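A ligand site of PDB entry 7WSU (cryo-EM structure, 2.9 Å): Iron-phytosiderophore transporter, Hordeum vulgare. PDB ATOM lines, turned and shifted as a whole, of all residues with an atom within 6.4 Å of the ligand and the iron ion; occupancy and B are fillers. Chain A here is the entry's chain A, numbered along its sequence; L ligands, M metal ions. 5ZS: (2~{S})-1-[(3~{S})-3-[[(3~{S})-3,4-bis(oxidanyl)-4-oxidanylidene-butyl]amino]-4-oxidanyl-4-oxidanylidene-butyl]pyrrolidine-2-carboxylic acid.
An oxygen (O5) of the ligand sits close to the backbone carbonyl oxygen (O) of Phe 130. O of Val 78 touches C4 of the ligand, 3.1 Å away. Gly 133 touches the ligand. Phe 134 touches the ligand (N to O6, 3.7 Å). Tyr 451 touches the ligand (CB to O2, 3.2 Å). Leu 486 touches the ligand (CD1 to O2, 3.1 Å). CG of Tyr 547 touches C10 of the ligand, at 3.6 Å. Hydrophobic or aromatic side chains that line the ligand: Val 78, Phe 130, Tyr 451, Leu 486, Tyr 547 and Tyr 551. Of the 26 residues printed, 13 come within 4 Å of the ligand. The nearest printed residue that does not touch the ligand is Ala 72 (4.4 Å).
N of Gly 135 lies within hydrogen-bond range of O6 of the ligand. O6 of the ligand sits at hydrogen-bond distance from OG of Ser 136 (2.8 Å). NZ of Lys 482 lies close to O5 of the ligand, 2.8 Å away. The side-chain amino group (NZ) of Lys 455 is in salt-bridge range of an oxygen (O4) of the ligand, 3.9 Å away. O of Gly 76 sits close to N2 of the ligand (3.1 Å). OH of Tyr 551 lies within hydrogen-bond range of O4 of the ligand (3.4 Å). The backbone NH (N) of Ser 136 sits at hydrogen-bond distance from an oxygen (O6) of the ligand.
The iron ion is bound by O1 of the ligand (1.9 Å), O5 of the ligand (2.0 Å), N2 of the ligand (2.0 Å), O7 of the ligand (2.0 Å), O3 of the ligand (2.1 Å) and N1 of the ligand (2.4 Å).
Merely in contact with the iron ion: Lys 482 (3.7 Å). Of the 26 residues printed, 1 comes within 4 Å of the iron ion. The nearest printed residue that does not touch the iron ion is Phe 130 (4.6 Å).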
ATOM      1  N   ALA A  72      -2.850  16.191   8.896  1.00  0.00           N
ATOM      2  CA  ALA A  72      -3.005  17.532   8.342  1.00  0.00           C
ATOM      3  C   ALA A  72      -3.111  18.577   9.451  1.00  0.00           C
ATOM      4  O   ALA A  72      -2.556  19.680   9.331  1.00  0.00           O
ATOM      5  CB  ALA A  72      -4.225  17.584   7.430  1.00  0.00           C
ATOM      6  N   LEU A  73      -3.822  18.255  10.532  1.00  0.00           N
ATOM      7  CA  LEU A  73      -4.053  19.207  11.615  1.00  0.00           C
ATOM      8  C   LEU A  73      -2.919  19.233  12.634  1.00  0.00           C
ATOM      9  O   LEU A  73      -2.986  20.026  13.580  1.00  0.00           O
ATOM     10  CB  LEU A  73      -5.366  18.880  12.332  1.00  0.00           C
ATOM     11  CG  LEU A  73      -6.639  18.868  11.470  1.00  0.00           C
ATOM     12  CD1 LEU A  73      -7.796  18.279  12.257  1.00  0.00           C
ATOM     13  CD2 LEU A  73      -6.964  20.263  10.987  1.00  0.00           C
ATOM     14  N   THR A  75       0.832  18.383  11.525  1.00  0.00           N
ATOM     15  CA  THR A  75       2.048  18.786  10.829  1.00  0.00           C
ATOM     16  C   THR A  75       1.797  19.351   9.438  1.00  0.00           C
ATOM     17  O   THR A  75       2.643  20.113   8.944  1.00  0.00           O
ATOM     18  CB  THR A  75       3.025  17.605  10.703  1.00  0.00           C
ATOM     19  OG1 THR A  75       2.415  16.554   9.952  1.00  0.00           O
ATOM     20  CG2 THR A  75       3.412  17.086  12.082  1.00  0.00           C
ATOM     21  N   GLY A  76       0.697  18.997   8.775  1.00  0.00           N
ATOM     22  CA  GLY A  76       0.417  19.470   7.445  1.00  0.00           C
ATOM     23  C   GLY A  76       1.132  18.710   6.345  1.00  0.00           C
ATOM     24  O   GLY A  76       0.960  19.060   5.163  1.00  0.00           O
ATOM     25  N   LEU A  77       1.919  17.687   6.673  1.00  0.00           N
ATOM     26  CA  LEU A  77       2.645  16.900   5.690  1.00  0.00           C
ATOM     27  C   LEU A  77       1.850  15.613   5.423  1.00  0.00           C
ATOM     28  O   LEU A  77       2.191  14.528   5.891  1.00  0.00           O
ATOM     29  CB  LEU A  77       4.061  16.602   6.168  1.00  0.00           C
ATOM     30  CG  LEU A  77       4.866  17.789   6.678  1.00  0.00           C
ATOM     31  CD1 LEU A  77       6.173  17.329   7.308  1.00  0.00           C
ATOM     32  CD2 LEU A  77       5.137  18.783   5.556  1.00  0.00           C
ATOM     33  N   VAL A  78       0.773  15.768   4.660  1.00  0.00           N
ATOM     34  CA  VAL A  78      -0.066  14.632   4.278  1.00  0.00           C
ATOM     35  C   VAL A  78       0.702  13.762   3.290  1.00  0.00           C
ATOM     36  O   VAL A  78       1.232  14.273   2.300  1.00  0.00           O
ATOM     37  CB  VAL A  78      -1.405  15.103   3.688  1.00  0.00           C
ATOM     38  CG1 VAL A  78      -2.151  13.939   3.068  1.00  0.00           C
ATOM     39  CG2 VAL A  78      -2.252  15.778   4.753  1.00  0.00           C
ATOM     40  N   PRO A  79       0.798  12.457   3.531  1.00  0.00           N
ATOM     41  CA  PRO A  79       1.547  11.587   2.620  1.00  0.00           C
ATOM     42  C   PRO A  79       0.645  11.003   1.536  1.00  0.00           C
ATOM     43  O   PRO A  79      -0.580  11.032   1.623  1.00  0.00           O
ATOM     44  CB  PRO A  79       2.049  10.492   3.567  1.00  0.00           C
ATOM     45  CG  PRO A  79       0.949  10.359   4.561  1.00  0.00           C
ATOM     46  CD  PRO A  79       0.348  11.739   4.737  1.00  0.00           C
ATOM     47  N   THR A  80       1.290  10.454   0.513  1.00  0.00           N
ATOM     48  CA  THR A  80       0.584   9.783  -0.567  1.00  0.00           C
ATOM     49  C   THR A  80       0.255   8.353  -0.152  1.00  0.00           C
ATOM     50  O   THR A  80       1.142   7.585   0.225  1.00  0.00           O
ATOM     51  CB  THR A  80       1.413   9.781  -1.848  1.00  0.00           C
ATOM     52  OG1 THR A  80       1.679  11.133  -2.242  1.00  0.00           O
ATOM     53  CG2 THR A  80       0.660   9.069  -2.965  1.00  0.00           C
ATOM     54  N   ALA A 129     -10.239  14.998   1.850  1.00  0.00           N
ATOM     55  CA  ALA A 129      -9.767  15.418   3.168  1.00  0.00           C
ATOM     56  C   ALA A 129      -8.659  16.454   3.063  1.00  0.00           C
ATOM     57  O   ALA A 129      -8.638  17.435   3.819  1.00  0.00           O
ATOM     58  CB  ALA A 129      -9.309  14.202   3.970  1.00  0.00           C
ATOM     59  N   PHE A 130      -7.712  16.257   2.143  1.00  0.00           N
ATOM     60  CA  PHE A 130      -6.626  17.207   1.956  1.00  0.00           C
ATOM     61  C   PHE A 130      -6.777  18.075   0.710  1.00  0.00           C
ATOM     62  O   PHE A 130      -6.201  19.169   0.671  1.00  0.00           O
ATOM     63  CB  PHE A 130      -5.275  16.491   1.918  1.00  0.00           C
ATOM     64  CG  PHE A 130      -5.072  15.621   0.705  1.00  0.00           C
ATOM     65  CD1 PHE A 130      -4.446  16.122  -0.426  1.00  0.00           C
ATOM     66  CD2 PHE A 130      -5.473  14.299   0.714  1.00  0.00           C
ATOM     67  CE1 PHE A 130      -4.257  15.326  -1.539  1.00  0.00           C
ATOM     68  CE2 PHE A 130      -5.276  13.494  -0.391  1.00  0.00           C
ATOM     69  CZ  PHE A 130      -4.666  14.014  -1.524  1.00  0.00           C
ATOM     70  N   ALA A 131      -7.531  17.625  -0.291  1.00  0.00           N
ATOM     71  CA  ALA A 131      -7.811  18.471  -1.448  1.00  0.00           C
ATOM     72  C   ALA A 131      -8.795  19.591  -1.119  1.00  0.00           C
ATOM     73  O   ALA A 131      -8.775  20.619  -1.791  1.00  0.00           O
ATOM     74  CB  ALA A 131      -8.361  17.641  -2.601  1.00  0.00           C
ATOM     75  N   GLY A 132      -9.639  19.408  -0.111  1.00  0.00           N
ATOM     76  CA  GLY A 132     -10.586  20.420   0.300  1.00  0.00           C
ATOM     77  C   GLY A 132     -10.013  21.509   1.180  1.00  0.00           C
ATOM     78  O   GLY A 132     -10.744  22.421   1.563  1.00  0.00           O
ATOM     79  N   GLY A 133      -8.732  21.434   1.508  1.00  0.00           N
ATOM     80  CA  GLY A 133      -8.100  22.447   2.342  1.00  0.00           C
ATOM     81  C   GLY A 133      -8.617  22.480   3.764  1.00  0.00           C
ATOM     82  O   GLY A 133      -8.777  23.563   4.332  1.00  0.00           O
ATOM     83  N   PHE A 134      -8.861  21.308   4.361  1.00  0.00           N
ATOM     84  CA  PHE A 134      -9.358  21.274   5.733  1.00  0.00           C
ATOM     85  C   PHE A 134      -8.290  21.696   6.731  1.00  0.00           C
ATOM     86  O   PHE A 134      -8.613  22.288   7.760  1.00  0.00           O
ATOM     87  CB  PHE A 134      -9.877  19.874   6.071  1.00  0.00           C
ATOM     88  CG  PHE A 134     -11.261  19.615   5.558  1.00  0.00           C
ATOM     89  CD1 PHE A 134     -12.363  20.152   6.203  1.00  0.00           C
ATOM     90  CD2 PHE A 134     -11.464  18.831   4.449  1.00  0.00           C
ATOM     91  CE1 PHE A 134     -13.631  19.924   5.742  1.00  0.00           C
ATOM     92  CE2 PHE A 134     -12.746  18.584   3.981  1.00  0.00           C
ATOM     93  CZ  PHE A 134     -13.825  19.130   4.628  1.00  0.00           C
ATOM     94  N   GLY A 135      -7.026  21.392   6.447  1.00  0.00           N
ATOM     95  CA  GLY A 135      -5.936  21.793   7.299  1.00  0.00           C
ATOM     96  C   GLY A 135      -5.140  22.992   6.824  1.00  0.00           C
ATOM     97  O   GLY A 135      -4.267  23.465   7.557  1.00  0.00           O
ATOM     98  N   SER A 136      -5.398  23.487   5.616  1.00  0.00           N
ATOM     99  CA  SER A 136      -4.653  24.616   5.078  1.00  0.00           C
ATOM    100  C   SER A 136      -5.527  25.841   4.854  1.00  0.00           C
ATOM    101  O   SER A 136      -5.216  26.920   5.382  1.00  0.00           O
ATOM    102  CB  SER A 136      -3.962  24.209   3.771  1.00  0.00           C
ATOM    103  OG  SER A 136      -4.916  23.832   2.781  1.00  0.00           O
ATOM    104  N   THR A 137      -6.620  25.722   4.095  1.00  0.00           N
ATOM    105  CA  THR A 137      -7.392  26.890   3.679  1.00  0.00           C
ATOM    106  C   THR A 137      -8.684  27.058   4.462  1.00  0.00           C
ATOM    107  O   THR A 137      -8.943  28.143   4.998  1.00  0.00           O
ATOM    108  CB  THR A 137      -7.699  26.807   2.189  1.00  0.00           C
ATOM    109  OG1 THR A 137      -6.485  26.675   1.439  1.00  0.00           O
ATOM    110  CG2 THR A 137      -8.403  28.066   1.736  1.00  0.00           C
ATOM    111  N   ASN A 448       2.030  15.844  -8.729  1.00  0.00           N
ATOM    112  CA  ASN A 448       0.797  16.621  -8.776  1.00  0.00           C
ATOM    113  C   ASN A 448       1.059  18.020  -8.220  1.00  0.00           C
ATOM    114  O   ASN A 448       1.388  18.178  -7.039  1.00  0.00           O
ATOM    115  CB  ASN A 448      -0.297  15.922  -7.968  1.00  0.00           C
ATOM    116  CG  ASN A 448      -1.684  16.301  -8.436  1.00  0.00           C
ATOM    117  OD1 ASN A 448      -1.950  17.462  -8.760  1.00  0.00           O
ATOM    118  ND2 ASN A 448      -2.584  15.330  -8.465  1.00  0.00           N
ATOM    119  N   GLY A 450      -1.249  20.400  -8.082  1.00  0.00           N
ATOM    120  CA  GLY A 450      -2.548  21.022  -7.889  1.00  0.00           C
ATOM    121  C   GLY A 450      -2.579  22.042  -6.764  1.00  0.00           C
ATOM    122  O   GLY A 450      -3.216  23.095  -6.895  1.00  0.00           O
ATOM    123  N   TYR A 451      -1.908  21.752  -5.652  1.00  0.00           N
ATOM    124  CA  TYR A 451      -1.859  22.706  -4.556  1.00  0.00           C
ATOM    125  C   TYR A 451      -1.013  23.922  -4.878  1.00  0.00           C
ATOM    126  O   TYR A 451      -1.155  24.955  -4.212  1.00  0.00           O
ATOM    127  CB  TYR A 451      -1.352  22.034  -3.283  1.00  0.00           C
ATOM    128  CG  TYR A 451       0.158  21.890  -3.199  1.00  0.00           C
ATOM    129  CD1 TYR A 451       0.817  20.859  -3.858  1.00  0.00           C
ATOM    130  CD2 TYR A 451       0.911  22.774  -2.436  1.00  0.00           C
ATOM    131  CE1 TYR A 451       2.186  20.728  -3.781  1.00  0.00           C
ATOM    132  CE2 TYR A 451       2.278  22.644  -2.346  1.00  0.00           C
ATOM    133  CZ  TYR A 451       2.910  21.619  -3.022  1.00  0.00           C
ATOM    134  OH  TYR A 451       4.280  21.496  -2.938  1.00  0.00           O
ATOM    135  N   ASN A 452      -0.143  23.836  -5.878  1.00  0.00           N
ATOM    136  CA  ASN A 452       0.622  25.008  -6.318  1.00  0.00           C
ATOM    137  C   ASN A 452      -0.231  25.949  -7.160  1.00  0.00           C
ATOM    138  O   ASN A 452      -0.019  27.160  -7.121  1.00  0.00           O
ATOM    139  CB  ASN A 452       1.856  24.570  -7.093  1.00  0.00           C
ATOM    140  CG  ASN A 452       2.841  23.801  -6.223  1.00  0.00           C
ATOM    141  OD1 ASN A 452       3.334  24.324  -5.231  1.00  0.00           O
ATOM    142  ND2 ASN A 452       3.129  22.563  -6.610  1.00  0.00           N
ATOM    143  N   LYS A 455      -2.245  28.092  -4.668  1.00  0.00           N
ATOM    144  CA  LYS A 455      -1.497  29.202  -4.094  1.00  0.00           C
ATOM    145  C   LYS A 455      -1.456  30.401  -5.033  1.00  0.00           C
ATOM    146  O   LYS A 455      -1.588  31.545  -4.581  1.00  0.00           O
ATOM    147  CB  LYS A 455      -0.082  28.759  -3.740  1.00  0.00           C
ATOM    148  CG  LYS A 455      -0.003  27.758  -2.605  1.00  0.00           C
ATOM    149  CD  LYS A 455       1.425  27.390  -2.291  1.00  0.00           C
ATOM    150  CE  LYS A 455       1.502  26.374  -1.170  1.00  0.00           C
ATOM    151  NZ  LYS A 455       2.907  25.998  -0.858  1.00  0.00           N
ATOM    152  N   LYS A 482      -7.891  24.938  -6.525  1.00  0.00           N
ATOM    153  CA  LYS A 482      -7.116  23.792  -6.088  1.00  0.00           C
ATOM    154  C   LYS A 482      -7.892  22.486  -6.202  1.00  0.00           C
ATOM    155  O   LYS A 482      -7.324  21.482  -6.637  1.00  0.00           O
ATOM    156  CB  LYS A 482      -6.640  23.991  -4.647  1.00  0.00           C
ATOM    157  CG  LYS A 482      -5.977  22.766  -4.030  1.00  0.00           C
ATOM    158  CD  LYS A 482      -5.448  23.073  -2.642  1.00  0.00           C
ATOM    159  CE  LYS A 482      -5.223  21.799  -1.843  1.00  0.00           C
ATOM    160  NZ  LYS A 482      -4.566  22.076  -0.547  1.00  0.00           N
ATOM    161  N   LEU A 486      -6.550  19.658  -8.565  1.00  0.00           N
ATOM    162  CA  LEU A 486      -5.935  18.521  -7.874  1.00  0.00           C
ATOM    163  C   LEU A 486      -6.735  17.246  -8.078  1.00  0.00           C
ATOM    164  O   LEU A 486      -6.152  16.169  -8.257  1.00  0.00           O
ATOM    165  CB  LEU A 486      -5.793  18.857  -6.397  1.00  0.00           C
ATOM    166  CG  LEU A 486      -4.864  18.038  -5.507  1.00  0.00           C
ATOM    167  CD1 LEU A 486      -4.271  18.947  -4.462  1.00  0.00           C
ATOM    168  CD2 LEU A 486      -5.629  16.928  -4.836  1.00  0.00           C
ATOM    169  N   TYR A 547      -0.014  25.340   8.319  1.00  0.00           N
ATOM    170  CA  TYR A 547      -0.414  25.845   7.019  1.00  0.00           C
ATOM    171  C   TYR A 547      -1.713  26.642   7.049  1.00  0.00           C
ATOM    172  O   TYR A 547      -2.007  27.355   6.085  1.00  0.00           O
ATOM    173  CB  TYR A 547      -0.545  24.689   6.022  1.00  0.00           C
ATOM    174  CG  TYR A 547       0.788  24.106   5.616  1.00  0.00           C
ATOM    175  CD1 TYR A 547       1.344  23.036   6.318  1.00  0.00           C
ATOM    176  CD2 TYR A 547       1.494  24.619   4.535  1.00  0.00           C
ATOM    177  CE1 TYR A 547       2.561  22.505   5.947  1.00  0.00           C
ATOM    178  CE2 TYR A 547       2.711  24.089   4.164  1.00  0.00           C
ATOM    179  CZ  TYR A 547       3.241  23.040   4.876  1.00  0.00           C
ATOM    180  OH  TYR A 547       4.458  22.510   4.505  1.00  0.00           O
ATOM    181  N   TYR A 551      -1.294  29.882   4.864  1.00  0.00           N
ATOM    182  CA  TYR A 551      -2.219  30.217   3.789  1.00  0.00           C
ATOM    183  C   TYR A 551      -2.967  31.516   4.078  1.00  0.00           C
ATOM    184  O   TYR A 551      -3.301  32.248   3.145  1.00  0.00           O
ATOM    185  CB  TYR A 551      -3.214  29.071   3.578  1.00  0.00           C
ATOM    186  CG  TYR A 551      -2.760  28.044   2.558  1.00  0.00           C
ATOM    187  CD1 TYR A 551      -1.784  27.112   2.877  1.00  0.00           C
ATOM    188  CD2 TYR A 551      -3.306  28.017   1.282  1.00  0.00           C
ATOM    189  CE1 TYR A 551      -1.372  26.174   1.959  1.00  0.00           C
ATOM    190  CE2 TYR A 551      -2.891  27.086   0.358  1.00  0.00           C
ATOM    191  CZ  TYR A 551      -1.925  26.164   0.696  1.00  0.00           C
ATOM    192  OH  TYR A 551      -1.510  25.233  -0.228  1.00  0.00           O
HETATM  193  N1  5ZS L   1      -0.169  19.037   0.654  1.00  0.00           N
HETATM  194  C2  5ZS L   1      -0.493  18.592  -0.555  1.00  0.00           C
HETATM  195  C3  5ZS L   1      -0.895  16.972  -0.368  1.00  0.00           C
HETATM  196  C4  5ZS L   1      -0.063  16.521   0.536  1.00  0.00           C
HETATM  197  C5  5ZS L   1       0.185  17.762   1.508  1.00  0.00           C
HETATM  198  C6  5ZS L   1       1.029  19.889   0.543  1.00  0.00           C
HETATM  199  C1  5ZS L   1      -1.673  19.325  -1.071  1.00  0.00           C
HETATM  200  C10 5ZS L   1      -1.295  21.501   4.147  1.00  0.00           C
HETATM  201  C11 5ZS L   1      -2.404  20.691   4.841  1.00  0.00           C
HETATM  202  C12 5ZS L   1      -3.251  19.863   3.838  1.00  0.00           C
HETATM  203  C13 5ZS L   1      -4.113  20.779   3.025  1.00  0.00           C
HETATM  204  C7  5ZS L   1       1.488  20.383   1.947  1.00  0.00           C
HETATM  205  C8  5ZS L   1       0.521  21.402   2.548  1.00  0.00           C
HETATM  206  C9  5ZS L   1       0.085  22.372   1.474  1.00  0.00           C
HETATM  207  N2  5ZS L   1      -0.649  20.695   3.093  1.00  0.00           N
HETATM  208  O1  5ZS L   1      -2.243  20.190  -0.377  1.00  0.00           O
HETATM  209  O2  5ZS L   1      -2.103  19.063  -2.226  1.00  0.00           O
HETATM  210  O3  5ZS L   1      -1.101  22.366   1.054  1.00  0.00           O
HETATM  211  O4  5ZS L   1       0.913  23.190   0.995  1.00  0.00           O
HETATM  212  O5  5ZS L   1      -3.701  21.227   1.928  1.00  0.00           O
HETATM  213  O6  5ZS L   1      -5.253  21.102   3.448  1.00  0.00           O
HETATM  214  O7  5ZS L   1      -2.405  19.154   2.974  1.00  0.00           O
HETATM  215 FE    FE M   1      -1.917  20.500   1.519  1.00  0.00          FE
